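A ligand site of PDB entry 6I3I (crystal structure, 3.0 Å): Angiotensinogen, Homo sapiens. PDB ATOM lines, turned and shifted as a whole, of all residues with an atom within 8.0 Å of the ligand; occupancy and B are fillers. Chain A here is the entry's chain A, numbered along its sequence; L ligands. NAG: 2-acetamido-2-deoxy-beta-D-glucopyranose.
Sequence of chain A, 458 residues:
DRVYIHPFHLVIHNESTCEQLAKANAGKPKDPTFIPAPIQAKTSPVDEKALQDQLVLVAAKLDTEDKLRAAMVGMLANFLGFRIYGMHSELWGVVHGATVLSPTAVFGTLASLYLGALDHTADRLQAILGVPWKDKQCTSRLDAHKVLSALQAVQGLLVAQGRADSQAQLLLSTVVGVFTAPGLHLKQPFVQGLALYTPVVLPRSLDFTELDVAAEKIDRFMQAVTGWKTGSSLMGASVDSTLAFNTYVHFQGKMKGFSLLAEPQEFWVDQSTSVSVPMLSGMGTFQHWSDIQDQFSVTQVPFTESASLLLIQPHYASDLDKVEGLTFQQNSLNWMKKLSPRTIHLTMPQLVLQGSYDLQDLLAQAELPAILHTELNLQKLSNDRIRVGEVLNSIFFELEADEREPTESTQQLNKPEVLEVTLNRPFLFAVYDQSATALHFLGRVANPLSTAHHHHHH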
ATOM      1  N   ILE A  12      26.830  -5.574  20.499  1.00  0.00           N
ATOM      2  CA  ILE A  12      28.104  -5.273  21.142  1.00  0.00           C
ATOM      3  C   ILE A  12      27.833  -4.906  22.611  1.00  0.00           C
ATOM      4  O   ILE A  12      26.696  -4.589  22.977  1.00  0.00           O
ATOM      5  CB  ILE A  12      28.875  -4.162  20.396  1.00  0.00           C
ATOM      6  CG1 ILE A  12      28.070  -2.859  20.297  1.00  0.00           C
ATOM      7  CG2 ILE A  12      29.313  -4.650  19.028  1.00  0.00           C
ATOM      8  CD1 ILE A  12      28.871  -1.672  19.808  1.00  0.00           C
ATOM      9  N   HIS A  13      28.880  -4.969  23.436  1.00  0.00           N
ATOM     10  CA  HIS A  13      28.815  -4.569  24.841  1.00  0.00           C
ATOM     11  C   HIS A  13      28.469  -3.082  24.947  1.00  0.00           C
ATOM     12  O   HIS A  13      28.643  -2.328  23.989  1.00  0.00           O
ATOM     13  CB  HIS A  13      30.139  -4.824  25.557  1.00  0.00           C
ATOM     14  CG  HIS A  13      30.577  -6.252  25.644  1.00  0.00           C
ATOM     15  ND1 HIS A  13      31.738  -6.703  25.040  1.00  0.00           N
ATOM     16  CD2 HIS A  13      30.044  -7.320  26.277  1.00  0.00           C
ATOM     17  CE1 HIS A  13      31.895  -7.983  25.283  1.00  0.00           C
ATOM     18  NE2 HIS A  13      30.869  -8.393  26.040  1.00  0.00           N
ATOM     19  N   ASN A  14      27.991  -2.666  26.131  1.00  0.00           N
ATOM     20  CA  ASN A  14      27.745  -1.263  26.447  1.00  0.00           C
ATOM     21  C   ASN A  14      28.442  -0.922  27.772  1.00  0.00           C
ATOM     22  O   ASN A  14      28.969  -1.806  28.436  1.00  0.00           O
ATOM     23  CB  ASN A  14      26.252  -0.913  26.429  1.00  0.00           C
ATOM     24  CG  ASN A  14      25.392  -1.892  27.197  1.00  0.00           C
ATOM     25  OD1 ASN A  14      25.859  -2.571  28.112  1.00  0.00           O
ATOM     26  ND2 ASN A  14      24.122  -1.971  26.836  1.00  0.00           N
ATOM     27  N   GLU A  15      28.411   0.368  28.135  1.00  0.00           N
ATOM     28  CA  GLU A  15      29.237   0.965  29.209  1.00  0.00           C
ATOM     29  C   GLU A  15      29.076   0.179  30.515  1.00  0.00           C
ATOM     30  O   GLU A  15      30.070  -0.221  31.120  1.00  0.00           O
ATOM     31  CB  GLU A  15      28.849   2.431  29.421  1.00  0.00           C
ATOM     32  CG  GLU A  15      29.201   3.333  28.249  1.00  0.00           C
ATOM     33  CD  GLU A  15      28.525   4.701  28.281  1.00  0.00           C
ATOM     34  OE1 GLU A  15      28.386   5.266  29.383  1.00  0.00           O
ATOM     35  OE2 GLU A  15      28.117   5.182  27.200  1.00  0.00           O
ATOM     36  N   SER A  16      27.818  -0.034  30.934  1.00  0.00           N
ATOM     37  CA  SER A  16      27.493  -0.712  32.191  1.00  0.00           C
ATOM     38  C   SER A  16      28.040  -2.143  32.190  1.00  0.00           C
ATOM     39  O   SER A  16      28.655  -2.583  33.160  1.00  0.00           O
ATOM     40  CB  SER A  16      26.009  -0.694  32.438  1.00  0.00           C
ATOM     41  OG  SER A  16      25.318  -1.435  31.442  1.00  0.00           O
ATOM     42  N   THR A  17      27.806  -2.856  31.077  1.00  0.00           N
ATOM     43  CA  THR A  17      28.232  -4.246  30.900  1.00  0.00           C
ATOM     44  C   THR A  17      29.762  -4.337  30.877  1.00  0.00           C
ATOM     45  O   THR A  17      30.351  -5.186  31.551  1.00  0.00           O
ATOM     46  CB  THR A  17      27.634  -4.853  29.629  1.00  0.00           C
ATOM     47  OG1 THR A  17      26.225  -4.646  29.661  1.00  0.00           O
ATOM     48  CG2 THR A  17      27.939  -6.324  29.468  1.00  0.00           C
ATOM     49  N   CYS A  18      30.393  -3.458  30.098  1.00  0.00           N
ATOM     50  CA  CYS A  18      31.840  -3.523  29.829  1.00  0.00           C
ATOM     51  C   CYS A  18      32.652  -3.109  31.061  1.00  0.00           C
ATOM     52  O   CYS A  18      32.171  -2.384  31.936  1.00  0.00           O
ATOM     53  CB  CYS A  18      32.244  -2.635  28.667  1.00  0.00           C
ATOM     54  SG  CYS A  18      32.631  -3.567  27.158  1.00  0.00           S
ATOM     55  N   GLU A  65      13.100  -3.913  21.959  1.00  0.00           N
ATOM     56  CA  GLU A  65      14.546  -3.879  21.730  1.00  0.00           C
ATOM     57  C   GLU A  65      15.039  -5.286  21.398  1.00  0.00           C
ATOM     58  O   GLU A  65      15.797  -5.477  20.437  1.00  0.00           O
ATOM     59  CB  GLU A  65      15.279  -3.309  22.947  1.00  0.00           C
ATOM     60  CG  GLU A  65      16.670  -2.793  22.626  1.00  0.00           C
ATOM     61  CD  GLU A  65      17.457  -2.308  23.826  1.00  0.00           C
ATOM     62  OE1 GLU A  65      17.601  -3.082  24.791  1.00  0.00           O
ATOM     63  OE2 GLU A  65      17.916  -1.138  23.795  1.00  0.00           O
ATOM     64  N   ARG A  69      16.988  -6.890  18.009  1.00  0.00           N
ATOM     65  CA  ARG A  69      18.249  -7.620  18.143  1.00  0.00           C
ATOM     66  C   ARG A  69      18.128  -8.969  17.418  1.00  0.00           C
ATOM     67  O   ARG A  69      19.079  -9.395  16.761  1.00  0.00           O
ATOM     68  CB  ARG A  69      18.600  -7.809  19.621  1.00  0.00           C
ATOM     69  CG  ARG A  69      20.012  -8.342  19.850  1.00  0.00           C
ATOM     70  CD  ARG A  69      20.349  -8.503  21.314  1.00  0.00           C
ATOM     71  NE  ARG A  69      20.484  -7.220  21.997  1.00  0.00           N
ATOM     72  CZ  ARG A  69      19.611  -6.719  22.869  1.00  0.00           C
ATOM     73  NH1 ARG A  69      18.551  -7.420  23.223  1.00  0.00           N
ATOM     74  NH2 ARG A  69      19.819  -5.524  23.387  1.00  0.00           N
ATOM     75  N   ASP A 143      29.029  -8.847  22.255  1.00  0.00           N
ATOM     76  CA  ASP A 143      28.421  -9.362  23.484  1.00  0.00           C
ATOM     77  C   ASP A 143      27.798 -10.725  23.168  1.00  0.00           C
ATOM     78  O   ASP A 143      26.645 -10.801  22.741  1.00  0.00           O
ATOM     79  CB  ASP A 143      27.403  -8.360  24.049  1.00  0.00           C
ATOM     80  CG  ASP A 143      26.989  -8.647  25.487  1.00  0.00           C
ATOM     81  OD1 ASP A 143      27.111  -9.811  25.911  1.00  0.00           O
ATOM     82  OD2 ASP A 143      26.549  -7.695  26.164  1.00  0.00           O
ATOM     83  N   HIS A 145      26.650 -13.071  24.918  1.00  0.00           N
ATOM     84  CA  HIS A 145      25.412 -13.297  25.671  1.00  0.00           C
ATOM     85  C   HIS A 145      24.210 -12.757  24.887  1.00  0.00           C
ATOM     86  O   HIS A 145      23.193 -13.449  24.753  1.00  0.00           O
ATOM     87  CB  HIS A 145      25.518 -12.671  27.064  1.00  0.00           C
ATOM     88  CG  HIS A 145      26.404 -13.434  27.987  1.00  0.00           C
ATOM     89  ND1 HIS A 145      26.203 -13.466  29.351  1.00  0.00           N
ATOM     90  CD2 HIS A 145      27.488 -14.214  27.742  1.00  0.00           C
ATOM     91  CE1 HIS A 145      27.121 -14.218  29.913  1.00  0.00           C
ATOM     92  NE2 HIS A 145      27.923 -14.694  28.953  1.00  0.00           N
ATOM     93  N   LYS A 146      24.336 -11.535  24.377  1.00  0.00           N
ATOM     94  CA  LYS A 146      23.270 -10.879  23.628  1.00  0.00           C
ATOM     95  C   LYS A 146      23.078 -11.576  22.272  1.00  0.00           C
ATOM     96  O   LYS A 146      21.951 -11.699  21.806  1.00  0.00           O
ATOM     97  CB  LYS A 146      23.579  -9.376  23.476  1.00  0.00           C
ATOM     98  CG  LYS A 146      23.361  -8.575  24.757  1.00  0.00           C
ATOM     99  CD  LYS A 146      23.684  -7.112  24.653  1.00  0.00           C
ATOM    100  CE  LYS A 146      23.429  -6.379  25.959  1.00  0.00           C
ATOM    101  NZ  LYS A 146      24.053  -5.040  25.982  1.00  0.00           N
ATOM    102  N   SER A 149      21.483 -15.260  23.035  1.00  0.00           N
ATOM    103  CA  SER A 149      20.082 -15.107  23.445  1.00  0.00           C
ATOM    104  C   SER A 149      19.229 -14.645  22.264  1.00  0.00           C
ATOM    105  O   SER A 149      18.096 -15.088  22.109  1.00  0.00           O
ATOM    106  CB  SER A 149      19.958 -14.162  24.618  1.00  0.00           C
ATOM    107  OG  SER A 149      20.185 -12.821  24.212  1.00  0.00           O
HETATM  108  C1  NAG L   1      23.039  -3.605  29.481  1.00  0.00           C
HETATM  109  C2  NAG L   1      21.947  -2.804  30.189  1.00  0.00           C
HETATM  110  C3  NAG L   1      21.420  -3.574  31.393  1.00  0.00           C
HETATM  111  C4  NAG L   1      21.033  -4.997  31.001  1.00  0.00           C
HETATM  112  C5  NAG L   1      22.201  -5.683  30.308  1.00  0.00           C
HETATM  113  C6  NAG L   1      21.865  -7.111  29.862  1.00  0.00           C
HETATM  114  C7  NAG L   1      22.593  -0.477  29.725  1.00  0.00           C
HETATM  115  C8  NAG L   1      23.176   0.787  30.292  1.00  0.00           C
HETATM  116  N2  NAG L   1      22.477  -1.499  30.580  1.00  0.00           N
HETATM  117  O3  NAG L   1      20.275  -2.906  31.936  1.00  0.00           O
HETATM  118  O4  NAG L   1      20.616  -5.717  32.167  1.00  0.00           O
HETATM  119  O5  NAG L   1      22.585  -4.923  29.159  1.00  0.00           O
HETATM  120  O6  NAG L   1      23.042  -7.780  29.412  1.00  0.00           O
HETATM  121  O7  NAG L   1      22.268  -0.551  28.553  1.00  0.00           O
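Residues that only touch the ligand: Thr 17 (3.4 Å) and Lys 146 (3.5 Å).
The side-chain hydroxyl (OG1) of Thr 17 lies within hydrogen-bond range of the side-chain amide oxygen (OD1) of Asn 14 (2.6 Å). The side-chain amide nitrogen (ND2) of Asn 14 sits close to the side-chain amino group (NZ) of Lys 146 (3.2 Å). The backbone carbonyl oxygen (O) of Lys 146 lies within hydrogen-bond range of the side-chain hydroxyl (OG) of Ser 149 (3.2 Å). The side-chain amino group (NZ) of Lys 146 lies within salt-bridge range of the side-chain carboxylate (OD2) of Asp 143 (3.6 Å).
An oxygen (O7) of the ligand lies within hydrogen-bond range of the side-chain amide nitrogen (ND2) of Asn 14 (2.9 Å). N2 of the ligand lies within hydrogen-bond range of OG of Ser 16 (3.0 Å).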
